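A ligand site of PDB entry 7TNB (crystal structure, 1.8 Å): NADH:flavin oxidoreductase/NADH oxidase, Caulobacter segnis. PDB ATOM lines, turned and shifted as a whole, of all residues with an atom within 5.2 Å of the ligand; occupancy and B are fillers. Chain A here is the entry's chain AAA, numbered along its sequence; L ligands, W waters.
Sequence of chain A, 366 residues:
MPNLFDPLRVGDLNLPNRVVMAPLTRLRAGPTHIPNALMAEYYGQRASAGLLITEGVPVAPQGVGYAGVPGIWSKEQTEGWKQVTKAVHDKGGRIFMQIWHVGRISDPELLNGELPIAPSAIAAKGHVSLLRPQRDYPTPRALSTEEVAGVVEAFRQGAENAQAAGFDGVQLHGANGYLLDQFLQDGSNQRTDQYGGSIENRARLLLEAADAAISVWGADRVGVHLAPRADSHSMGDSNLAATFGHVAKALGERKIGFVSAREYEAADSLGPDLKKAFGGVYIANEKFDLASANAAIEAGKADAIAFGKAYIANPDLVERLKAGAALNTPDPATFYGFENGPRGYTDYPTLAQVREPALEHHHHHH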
ATOM      1  N   ALA A  22      19.287   2.181 -14.141  1.00  0.00           N
ATOM      2  CA  ALA A  22      19.667   2.233 -12.725  1.00  0.00           C
ATOM      3  C   ALA A  22      18.713   3.149 -11.965  1.00  0.00           C
ATOM      4  O   ALA A  22      18.182   4.111 -12.492  1.00  0.00           O
ATOM      5  CB  ALA A  22      21.073   2.699 -12.591  1.00  0.00           C
ATOM      6  N   PRO A  23      18.519   2.884 -10.662  1.00  0.00           N
ATOM      7  CA  PRO A  23      17.692   3.724  -9.810  1.00  0.00           C
ATOM      8  C   PRO A  23      18.348   5.106  -9.635  1.00  0.00           C
ATOM      9  O   PRO A  23      19.567   5.200  -9.319  1.00  0.00           O
ATOM     10  CB  PRO A  23      17.626   2.924  -8.476  1.00  0.00           C
ATOM     11  CG  PRO A  23      18.843   2.010  -8.494  1.00  0.00           C
ATOM     12  CD  PRO A  23      19.063   1.708  -9.958  1.00  0.00           C
ATOM     13  N   LEU A  24      17.579   6.145  -9.884  1.00  0.00           N
ATOM     14  CA  LEU A  24      18.113   7.526  -9.880  1.00  0.00           C
ATOM     15  C   LEU A  24      17.158   8.498  -9.176  1.00  0.00           C
ATOM     16  O   LEU A  24      16.139   8.890  -9.759  1.00  0.00           O
ATOM     17  CB  LEU A  24      18.376   7.972 -11.331  1.00  0.00           C
ATOM     18  CG  LEU A  24      19.400   7.150 -12.080  1.00  0.00           C
ATOM     19  CD1 LEU A  24      19.145   7.307 -13.576  1.00  0.00           C
ATOM     20  CD2 LEU A  24      20.834   7.552 -11.678  1.00  0.00           C
ATOM     21  N   THR A  25      17.563   8.921  -7.979  1.00  0.00           N
ATOM     22  CA  THR A  25      16.888  10.000  -7.227  1.00  0.00           C
ATOM     23  C   THR A  25      16.960  11.282  -8.052  1.00  0.00           C
ATOM     24  O   THR A  25      18.086  11.678  -8.414  1.00  0.00           O
ATOM     25  CB  THR A  25      17.522  10.169  -5.860  1.00  0.00           C
ATOM     26  OG1 THR A  25      17.207   9.024  -5.069  1.00  0.00           O
ATOM     27  CG2 THR A  25      16.998  11.373  -5.124  1.00  0.00           C
ATOM     28  N   ARG A  26      15.811  11.891  -8.305  1.00  0.00           N
ATOM     29  CA  ARG A  26      15.720  13.162  -9.066  1.00  0.00           C
ATOM     30  C   ARG A  26      14.956  14.240  -8.282  1.00  0.00           C
ATOM     31  O   ARG A  26      15.092  15.425  -8.668  1.00  0.00           O
ATOM     32  CB  ARG A  26      15.106  12.942 -10.452  1.00  0.00           C
ATOM     33  CG  ARG A  26      15.649  11.736 -11.211  1.00  0.00           C
ATOM     34  CD  ARG A  26      17.154  11.800 -11.535  1.00  0.00           C
ATOM     35  NE  ARG A  26      17.496  13.075 -12.135  1.00  0.00           N
ATOM     36  CZ  ARG A  26      17.313  13.386 -13.419  1.00  0.00           C
ATOM     37  NH1 ARG A  26      16.859  12.471 -14.266  1.00  0.00           N
ATOM     38  NH2 ARG A  26      17.583  14.602 -13.868  1.00  0.00           N
ATOM     39  N   GLU A  55      13.873   5.622  -9.262  1.00  0.00           N
ATOM     40  CA  GLU A  55      14.422   6.341  -8.098  1.00  0.00           C
ATOM     41  C   GLU A  55      14.042   5.624  -6.799  1.00  0.00           C
ATOM     42  O   GLU A  55      12.939   5.074  -6.689  1.00  0.00           O
ATOM     43  CB  GLU A  55      13.840   7.767  -8.058  1.00  0.00           C
ATOM     44  CG  GLU A  55      12.332   7.813  -7.845  1.00  0.00           C
ATOM     45  CD  GLU A  55      11.641   8.995  -8.525  1.00  0.00           C
ATOM     46  OE1 GLU A  55      11.580  10.090  -7.877  1.00  0.00           O
ATOM     47  OE2 GLU A  55      11.233   8.852  -9.729  1.00  0.00           O
ATOM     48  N   GLY A  56      14.911   5.697  -5.802  1.00  0.00           N
ATOM     49  CA  GLY A  56      14.558   5.228  -4.459  1.00  0.00           C
ATOM     50  C   GLY A  56      13.240   5.848  -4.005  1.00  0.00           C
ATOM     51  O   GLY A  56      12.958   7.049  -4.250  1.00  0.00           O
ATOM     52  N   GLN A  98      12.124   0.824  -6.813  1.00  0.00           N
ATOM     53  CA  GLN A  98      13.138   0.711  -5.728  1.00  0.00           C
ATOM     54  C   GLN A  98      12.492   1.209  -4.433  1.00  0.00           C
ATOM     55  O   GLN A  98      12.171   2.378  -4.363  1.00  0.00           O
ATOM     56  CB  GLN A  98      14.457   1.415  -6.008  1.00  0.00           C
ATOM     57  CG  GLN A  98      15.452   1.204  -4.883  1.00  0.00           C
ATOM     58  CD  GLN A  98      16.732   1.966  -5.057  1.00  0.00           C
ATOM     59  OE1 GLN A  98      16.747   3.167  -4.915  1.00  0.00           O
ATOM     60  NE2 GLN A  98      17.793   1.259  -5.364  1.00  0.00           N
ATOM     61  N   TRP A 100      12.770   1.839  -0.293  1.00  0.00           N
ATOM     62  CA  TRP A 100      13.901   2.506   0.376  1.00  0.00           C
ATOM     63  C   TRP A 100      13.598   2.980   1.789  1.00  0.00           C
ATOM     64  O   TRP A 100      12.445   3.400   2.079  1.00  0.00           O
ATOM     65  CB  TRP A 100      14.221   3.724  -0.480  1.00  0.00           C
ATOM     66  CG  TRP A 100      15.495   4.445  -0.248  1.00  0.00           C
ATOM     67  CD1 TRP A 100      16.663   4.028   0.326  1.00  0.00           C
ATOM     68  CD2 TRP A 100      15.707   5.765  -0.736  1.00  0.00           C
ATOM     69  NE1 TRP A 100      17.592   5.031   0.191  1.00  0.00           N
ATOM     70  CE2 TRP A 100      17.036   6.101  -0.451  1.00  0.00           C
ATOM     71  CE3 TRP A 100      14.902   6.680  -1.426  1.00  0.00           C
ATOM     72  CZ2 TRP A 100      17.577   7.334  -0.841  1.00  0.00           C
ATOM     73  CZ3 TRP A 100      15.446   7.889  -1.850  1.00  0.00           C
ATOM     74  CH2 TRP A 100      16.770   8.196  -1.554  1.00  0.00           C
ATOM     75  N   HIS A 173      16.294  -1.420  -1.791  1.00  0.00           N
ATOM     76  CA  HIS A 173      17.501  -0.593  -1.684  1.00  0.00           C
ATOM     77  C   HIS A 173      18.336  -1.152  -0.547  1.00  0.00           C
ATOM     78  O   HIS A 173      18.260  -0.593   0.594  1.00  0.00           O
ATOM     79  CB  HIS A 173      17.190   0.898  -1.511  1.00  0.00           C
ATOM     80  CG  HIS A 173      18.336   1.731  -1.948  1.00  0.00           C
ATOM     81  ND1 HIS A 173      19.644   1.267  -1.923  1.00  0.00           N
ATOM     82  CD2 HIS A 173      18.397   3.049  -2.275  1.00  0.00           C
ATOM     83  CE1 HIS A 173      20.444   2.225  -2.360  1.00  0.00           C
ATOM     84  NE2 HIS A 173      19.706   3.340  -2.562  1.00  0.00           N
ATOM     85  N   ALA A 175      21.622  -1.012  -0.571  1.00  0.00           N
ATOM     86  CA  ALA A 175      22.916  -0.468  -1.040  1.00  0.00           C
ATOM     87  C   ALA A 175      23.202   0.929  -0.442  1.00  0.00           C
ATOM     88  O   ALA A 175      22.435   1.430   0.401  1.00  0.00           O
ATOM     89  CB  ALA A 175      22.913  -0.463  -2.557  1.00  0.00           C
ATOM     90  N   ASN A 176      24.396   1.445  -0.746  1.00  0.00           N
ATOM     91  CA  ASN A 176      24.831   2.853  -0.619  1.00  0.00           C
ATOM     92  C   ASN A 176      24.665   3.366   0.824  1.00  0.00           C
ATOM     93  O   ASN A 176      24.432   4.567   0.974  1.00  0.00           O
ATOM     94  CB  ASN A 176      24.080   3.699  -1.630  1.00  0.00           C
ATOM     95  CG  ASN A 176      24.305   3.134  -3.010  1.00  0.00           C
ATOM     96  OD1 ASN A 176      25.300   2.423  -3.216  1.00  0.00           O
ATOM     97  ND2 ASN A 176      23.472   3.521  -3.944  1.00  0.00           N
ATOM     98  N   HIS A 225      19.244  -4.687  -4.479  1.00  0.00           N
ATOM     99  CA  HIS A 225      20.371  -3.822  -4.882  1.00  0.00           C
ATOM    100  C   HIS A 225      21.414  -3.780  -3.759  1.00  0.00           C
ATOM    101  O   HIS A 225      21.049  -3.556  -2.621  1.00  0.00           O
ATOM    102  CB  HIS A 225      19.818  -2.429  -5.199  1.00  0.00           C
ATOM    103  CG  HIS A 225      20.776  -1.583  -5.937  1.00  0.00           C
ATOM    104  ND1 HIS A 225      21.404  -2.028  -7.085  1.00  0.00           N
ATOM    105  CD2 HIS A 225      21.198  -0.317  -5.722  1.00  0.00           C
ATOM    106  CE1 HIS A 225      22.174  -1.062  -7.533  1.00  0.00           C
ATOM    107  NE2 HIS A 225      22.023   0.012  -6.750  1.00  0.00           N
ATOM    108  N   ARG A 262      25.732  -1.824  -7.541  1.00  0.00           N
ATOM    109  CA  ARG A 262      26.643  -0.708  -7.850  1.00  0.00           C
ATOM    110  C   ARG A 262      28.053  -1.152  -7.452  1.00  0.00           C
ATOM    111  O   ARG A 262      28.333  -1.235  -6.246  1.00  0.00           O
ATOM    112  CB  ARG A 262      26.263   0.591  -7.134  1.00  0.00           C
ATOM    113  CG  ARG A 262      27.214   1.712  -7.512  1.00  0.00           C
ATOM    114  CD  ARG A 262      26.976   2.987  -6.696  1.00  0.00           C
ATOM    115  NE  ARG A 262      27.110   2.799  -5.254  1.00  0.00           N
ATOM    116  CZ  ARG A 262      28.291   2.763  -4.591  1.00  0.00           C
ATOM    117  NH1 ARG A 262      29.433   2.922  -5.232  1.00  0.00           N
ATOM    118  NH2 ARG A 262      28.301   2.587  -3.286  1.00  0.00           N
ATOM    119  N   ASN A 285      26.721  -2.701 -12.618  1.00  0.00           N
ATOM    120  CA  ASN A 285      26.513  -1.241 -12.719  1.00  0.00           C
ATOM    121  C   ASN A 285      27.774  -0.554 -12.203  1.00  0.00           C
ATOM    122  O   ASN A 285      28.406  -1.080 -11.267  1.00  0.00           O
ATOM    123  CB  ASN A 285      25.290  -0.823 -11.898  1.00  0.00           C
ATOM    124  CG  ASN A 285      25.260   0.663 -11.594  1.00  0.00           C
ATOM    125  OD1 ASN A 285      25.500   1.083 -10.463  1.00  0.00           O
ATOM    126  ND2 ASN A 285      24.966   1.457 -12.612  1.00  0.00           N
ATOM    127  N   GLU A 286      27.985   0.662 -12.724  1.00  0.00           N
ATOM    128  CA  GLU A 286      28.900   1.696 -12.209  1.00  0.00           C
ATOM    129  C   GLU A 286      30.082   1.826 -13.173  1.00  0.00           C
ATOM    130  O   GLU A 286      30.933   0.935 -13.200  1.00  0.00           O
ATOM    131  CB  GLU A 286      29.396   1.451 -10.798  1.00  0.00           C
ATOM    132  CG  GLU A 286      30.071   2.682 -10.216  1.00  0.00           C
ATOM    133  CD  GLU A 286      30.400   2.608  -8.731  1.00  0.00           C
ATOM    134  OE1 GLU A 286      30.803   1.522  -8.283  1.00  0.00           O
ATOM    135  OE2 GLU A 286      30.217   3.631  -8.047  1.00  0.00           O
ATOM    136  N   LYS A 287      30.089   2.910 -13.935  1.00  0.00           N
ATOM    137  CA  LYS A 287      31.188   3.280 -14.864  1.00  0.00           C
ATOM    138  C   LYS A 287      31.244   2.305 -16.046  1.00  0.00           C
ATOM    139  O   LYS A 287      32.309   2.200 -16.679  1.00  0.00           O
ATOM    140  CB  LYS A 287      32.500   3.402 -14.082  1.00  0.00           C
ATOM    141  CG  LYS A 287      32.474   4.553 -13.079  1.00  0.00           C
ATOM    142  CD  LYS A 287      33.675   4.632 -12.165  1.00  0.00           C
ATOM    143  CE  LYS A 287      33.563   5.779 -11.165  1.00  0.00           C
ATOM    144  NZ  LYS A 287      34.794   5.911 -10.346  1.00  0.00           N
ATOM    145  N   PHE A 288      30.142   1.659 -16.413  1.00  0.00           N
ATOM    146  CA  PHE A 288      30.155   0.789 -17.623  1.00  0.00           C
ATOM    147  C   PHE A 288      29.989   1.658 -18.864  1.00  0.00           C
ATOM    148  O   PHE A 288      29.380   2.726 -18.784  1.00  0.00           O
ATOM    149  CB  PHE A 288      29.071  -0.287 -17.555  1.00  0.00           C
ATOM    150  CG  PHE A 288      29.480  -1.468 -16.740  1.00  0.00           C
ATOM    151  CD1 PHE A 288      29.409  -1.428 -15.347  1.00  0.00           C
ATOM    152  CD2 PHE A 288      30.018  -2.599 -17.342  1.00  0.00           C
ATOM    153  CE1 PHE A 288      29.815  -2.525 -14.591  1.00  0.00           C
ATOM    154  CE2 PHE A 288      30.440  -3.683 -16.575  1.00  0.00           C
ATOM    155  CZ  PHE A 288      30.337  -3.647 -15.206  1.00  0.00           C
ATOM    156  N   ALA A 306      23.129  -2.054 -15.787  1.00  0.00           N
ATOM    157  CA  ALA A 306      22.360  -0.840 -15.473  1.00  0.00           C
ATOM    158  C   ALA A 306      23.251   0.374 -15.689  1.00  0.00           C
ATOM    159  O   ALA A 306      24.439   0.331 -15.312  1.00  0.00           O
ATOM    160  CB  ALA A 306      21.813  -0.820 -14.071  1.00  0.00           C
ATOM    161  N   PHE A 307      22.679   1.406 -16.304  1.00  0.00           N
ATOM    162  CA  PHE A 307      23.334   2.688 -16.556  1.00  0.00           C
ATOM    163  C   PHE A 307      22.619   3.741 -15.731  1.00  0.00           C
ATOM    164  O   PHE A 307      21.372   3.763 -15.784  1.00  0.00           O
ATOM    165  CB  PHE A 307      23.298   2.996 -18.043  1.00  0.00           C
ATOM    166  CG  PHE A 307      24.051   2.023 -18.880  1.00  0.00           C
ATOM    167  CD1 PHE A 307      23.442   0.863 -19.376  1.00  0.00           C
ATOM    168  CD2 PHE A 307      25.395   2.227 -19.148  1.00  0.00           C
ATOM    169  CE1 PHE A 307      24.164  -0.061 -20.114  1.00  0.00           C
ATOM    170  CE2 PHE A 307      26.108   1.290 -19.905  1.00  0.00           C
ATOM    171  CZ  PHE A 307      25.494   0.153 -20.368  1.00  0.00           C
ATOM    172  N   GLY A 308      23.358   4.550 -14.972  1.00  0.00           N
ATOM    173  CA  GLY A 308      22.817   5.660 -14.167  1.00  0.00           C
ATOM    174  C   GLY A 308      22.900   6.966 -14.946  1.00  0.00           C
ATOM    175  O   GLY A 308      21.921   7.362 -15.613  1.00  0.00           O
ATOM    176  N   LYS A 309      24.033   7.633 -14.900  1.00  0.00           N
ATOM    177  CA  LYS A 309      24.171   9.014 -15.450  1.00  0.00           C
ATOM    178  C   LYS A 309      23.861   9.036 -16.968  1.00  0.00           C
ATOM    179  O   LYS A 309      23.238  10.021 -17.429  1.00  0.00           O
ATOM    180  CB  LYS A 309      25.561   9.521 -15.089  1.00  0.00           C
ATOM    181  CG  LYS A 309      25.669   9.997 -13.632  1.00  0.00           C
ATOM    182  CD  LYS A 309      27.019  10.577 -13.231  1.00  0.00           C
ATOM    183  CE  LYS A 309      28.130   9.600 -13.431  1.00  0.00           C
ATOM    184  NZ  LYS A 309      27.987   8.445 -12.516  1.00  0.00           N
ATOM    185  N   ALA A 310      24.209   7.974 -17.711  1.00  0.00           N
ATOM    186  CA  ALA A 310      23.888   7.901 -19.168  1.00  0.00           C
ATOM    187  C   ALA A 310      22.372   7.906 -19.380  1.00  0.00           C
ATOM    188  O   ALA A 310      21.941   8.420 -20.425  1.00  0.00           O
ATOM    189  CB  ALA A 310      24.481   6.698 -19.812  1.00  0.00           C
ATOM    190  N   ILE A 312      20.140   9.347 -17.288  1.00  0.00           N
ATOM    191  CA  ILE A 312      19.716  10.742 -17.020  1.00  0.00           C
ATOM    192  C   ILE A 312      19.699  11.498 -18.354  1.00  0.00           C
ATOM    193  O   ILE A 312      18.667  12.125 -18.694  1.00  0.00           O
ATOM    194  CB  ILE A 312      20.587  11.433 -15.971  1.00  0.00           C
ATOM    195  CG1 ILE A 312      20.398  10.761 -14.613  1.00  0.00           C
ATOM    196  CG2 ILE A 312      20.292  12.951 -15.953  1.00  0.00           C
ATOM    197  CD1 ILE A 312      21.267  11.297 -13.505  1.00  0.00           C
ATOM    198  N   PHE A 335      20.494  17.295 -11.950  1.00  0.00           N
ATOM    199  CA  PHE A 335      20.232  15.926 -11.422  1.00  0.00           C
ATOM    200  C   PHE A 335      19.103  15.997 -10.391  1.00  0.00           C
ATOM    201  O   PHE A 335      18.163  15.236 -10.458  1.00  0.00           O
ATOM    202  CB  PHE A 335      21.495  15.336 -10.813  1.00  0.00           C
ATOM    203  CG  PHE A 335      22.522  14.853 -11.797  1.00  0.00           C
ATOM    204  CD1 PHE A 335      22.334  15.027 -13.152  1.00  0.00           C
ATOM    205  CD2 PHE A 335      23.688  14.254 -11.340  1.00  0.00           C
ATOM    206  CE1 PHE A 335      23.284  14.579 -14.059  1.00  0.00           C
ATOM    207  CE2 PHE A 335      24.645  13.817 -12.242  1.00  0.00           C
ATOM    208  CZ  PHE A 335      24.436  13.969 -13.599  1.00  0.00           C
ATOM    209  N   TYR A 336      19.187  16.954  -9.467  1.00  0.00           N
ATOM    210  CA  TYR A 336      18.300  17.000  -8.270  1.00  0.00           C
ATOM    211  C   TYR A 336      17.491  18.293  -8.260  1.00  0.00           C
ATOM    212  O   TYR A 336      17.979  19.285  -8.727  1.00  0.00           O
ATOM    213  CB  TYR A 336      19.135  16.967  -7.000  1.00  0.00           C
ATOM    214  CG  TYR A 336      20.014  15.769  -6.884  1.00  0.00           C
ATOM    215  CD1 TYR A 336      19.447  14.530  -6.655  1.00  0.00           C
ATOM    216  CD2 TYR A 336      21.393  15.868  -7.003  1.00  0.00           C
ATOM    217  CE1 TYR A 336      20.240  13.400  -6.522  1.00  0.00           C
ATOM    218  CE2 TYR A 336      22.193  14.748  -6.879  1.00  0.00           C
ATOM    219  CZ  TYR A 336      21.619  13.519  -6.643  1.00  0.00           C
ATOM    220  OH  TYR A 336      22.403  12.418  -6.519  1.00  0.00           O
HETATM  221  N1  LIG L   1      21.281   4.484  -6.540  1.00  0.00           N
HETATM  222  C1  LIG L   1      20.227   3.904  -5.932  1.00  0.00           C
HETATM  223  O1  LIG L   1      20.274   2.673  -5.577  1.00  0.00           O
HETATM  224  N2  LIG L   1      19.096   4.583  -5.678  1.00  0.00           N
HETATM  225  C2  LIG L   1      18.961   5.943  -5.907  1.00  0.00           C
HETATM  226  O2  LIG L   1      17.855   6.497  -5.715  1.00  0.00           O
HETATM  227  C3  LIG L   1      20.031   6.597  -6.596  1.00  0.00           C
HETATM  228  N3  LIG L   1      19.931   7.890  -6.908  1.00  0.00           N
HETATM  229  C4  LIG L   1      20.929   8.421  -7.697  1.00  0.00           C
HETATM  230  C5  LIG L   1      20.814   9.737  -8.175  1.00  0.00           C
HETATM  231  C6  LIG L   1      21.739  10.299  -9.023  1.00  0.00           C
HETATM  232  C7  LIG L   1      21.540  11.721  -9.522  1.00  0.00           C
HETATM  233  C8  LIG L   1      22.864   9.568  -9.393  1.00  0.00           C
HETATM  234  C9  LIG L   1      23.909  10.160 -10.301  1.00  0.00           C
HETATM  235  C10 LIG L   1      23.023   8.286  -8.895  1.00  0.00           C
HETATM  236  C11 LIG L   1      22.066   7.679  -8.082  1.00  0.00           C
HETATM  237  N4  LIG L   1      22.188   6.383  -7.600  1.00  0.00           N
HETATM  238  C12 LIG L   1      21.177   5.775  -6.880  1.00  0.00           C
HETATM  239  C13 LIG L   1      23.326   5.574  -8.056  1.00  0.00           C
HETATM  240  C14 LIG L   1      23.043   4.985  -9.452  1.00  0.00           C
HETATM  241  O3  LIG L   1      21.977   3.994  -9.452  1.00  0.00           O
HETATM  242  C15 LIG L   1      24.312   4.311 -10.030  1.00  0.00           C
HETATM  243  O4  LIG L   1      24.728   3.213  -9.189  1.00  0.00           O
HETATM  244  C16 LIG L   1      25.495   5.246 -10.253  1.00  0.00           C
HETATM  245  O5  LIG L   1      25.057   6.406 -10.962  1.00  0.00           O
HETATM  246  C17 LIG L   1      26.655   4.620 -11.010  1.00  0.00           C
HETATM  247  O6  LIG L   1      26.231   4.177 -12.295  1.00  0.00           O
HETATM  248  P1  LIG L   1      26.699   4.986 -13.608  1.00  0.00           P
HETATM  249  O7  LIG L   1      28.248   5.061 -13.630  1.00  0.00           O
HETATM  250  O8  LIG L   1      26.080   4.234 -14.774  1.00  0.00           O
HETATM  251  O9  LIG L   1      26.113   6.350 -13.389  1.00  0.00           O
HETATM  252  O   HOH W   1      29.319   6.457 -15.396  1.00  0.00           O
HETATM  253  O   HOH W   2      25.931   5.576 -17.075  1.00  0.00           O
HETATM  254  O   HOH W   3      29.777   6.454 -11.751  1.00  0.00           O
HETATM  255  O   HOH W   4      27.373   8.799 -10.016  1.00  0.00           O
HETATM  256  O   HOH W   5      23.199   2.541  -6.911  1.00  0.00           O
HETATM  257  O   HOH W   6      25.043  10.506  -7.102  1.00  0.00           O
HETATM  258  O   HOH W   7      27.090   1.739 -15.252  1.00  0.00           O
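NE2 of His 225 sits close to O1 of the ligand (3.4 Å).
NZ of Lys 309 lies within salt-bridge range of O9 of the ligand (2.9 Å).
The backbone NH of Gly 308 sits at hydrogen-bond distance from an oxygen (O8) of the ligand (2.7 Å).
The side-chain amide oxygen (OD1) of Asn 285 lies within hydrogen-bond range of an oxygen (O4) of the ligand (2.6 Å).
A ring nitrogen (NE2) of His 173 sits at hydrogen-bond distance from an oxygen (O1) of the ligand, at 3.1 Å.
N of Lys 309 is in hydrogen-bond range of O9 of the ligand, 2.9 Å away.
An oxygen (O7) of the ligand lies within hydrogen-bond range of the backbone NH of Lys 287, 2.8 Å away.
O of Pro 23 sits at hydrogen-bond distance from O3 of the ligand (2.7 Å).
The backbone NH of Gly 56 is in hydrogen-bond range of an oxygen (O2) of the ligand (3.1 Å).
The side-chain amide oxygen (OE1) of Gln 98 lies within hydrogen-bond range of a nitrogen (N2) of the ligand (2.8 Å).
OG1 of Thr 25 lies within hydrogen-bond range of O2 of the ligand.
N of Thr 25 lies within hydrogen-bond range of N3 of the ligand, 2.8 Å away.
The backbone carbonyl oxygen of Phe 335 lies within hydrogen-bond range of the guanidinium group of Arg 26 (2.8 Å).
A ring nitrogen (ND1) of His 173 lies close to the backbone NH (N) of Ala 175 (3.3 Å).
The guanidinium group (NH1) of Arg 262 lies within salt-bridge range of the side-chain carboxylate (OE2) of Glu 286.
The backbone NH of Gly 56 sits close to the side-chain amide oxygen of Gln 98, at 3.2 Å.
The backbone carbonyl oxygen (O) of Phe 307 sits at hydrogen-bond distance from the backbone NH (N) of Ala 22 (3.1 Å).
The backbone carbonyl oxygen of His 225 lies within hydrogen-bond range of the backbone NH of Ala 175.
The backbone carbonyl oxygen of Ala 306 lies within hydrogen-bond range of the side-chain amide nitrogen of Asn 285, 3.0 Å away.
NE of Arg 262 sits at hydrogen-bond distance from OD1 of Asn 176, at 2.8 Å.
Ala 22 touches the ligand.
Leu 24 touches the ligand.
Asn 176 touches the ligand (ND2 to N1, 3.5 Å).
CG of Arg 262 touches O4 of the ligand, at 3.4 Å.
Glu 286 touches the ligand (CA to O6, 3.6 Å).
Phe 307 touches the ligand.
Phe 335 touches the ligand (CD2 to C7, 3.8 Å).
Tyr 336 touches the ligand.
18 residues have an atom within 4 Å of the ligand: Ala 22, Pro 23, Leu 24, Thr 25, Gly 56, Gln 98, His 173, Asn 176, His 225, Arg 262, Asn 285, Glu 286, Lys 287, Phe 307, Gly 308, Lys 309, Phe 335 and Tyr 336.
Water W2 lies within hydrogen-bond range of an oxygen (O8) of the ligand (2.7 Å), the backbone NH (N) of Ala 310 (3.0 Å) and the backbone NH (N) of Gly 308 (3.5 Å).
Water W5 lies within hydrogen-bond range of a nitrogen (N1) of the ligand, a ring nitrogen (NE2) of His 225 and the side-chain amide nitrogen (ND2) of Asn 176.
Water W3 lies within hydrogen-bond range of NZ of Lys 309 and O7 of the ligand.
Water W4 bridges NZ of Lys 309 (2.6 Å) and O5 of the ligand (3.5 Å).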
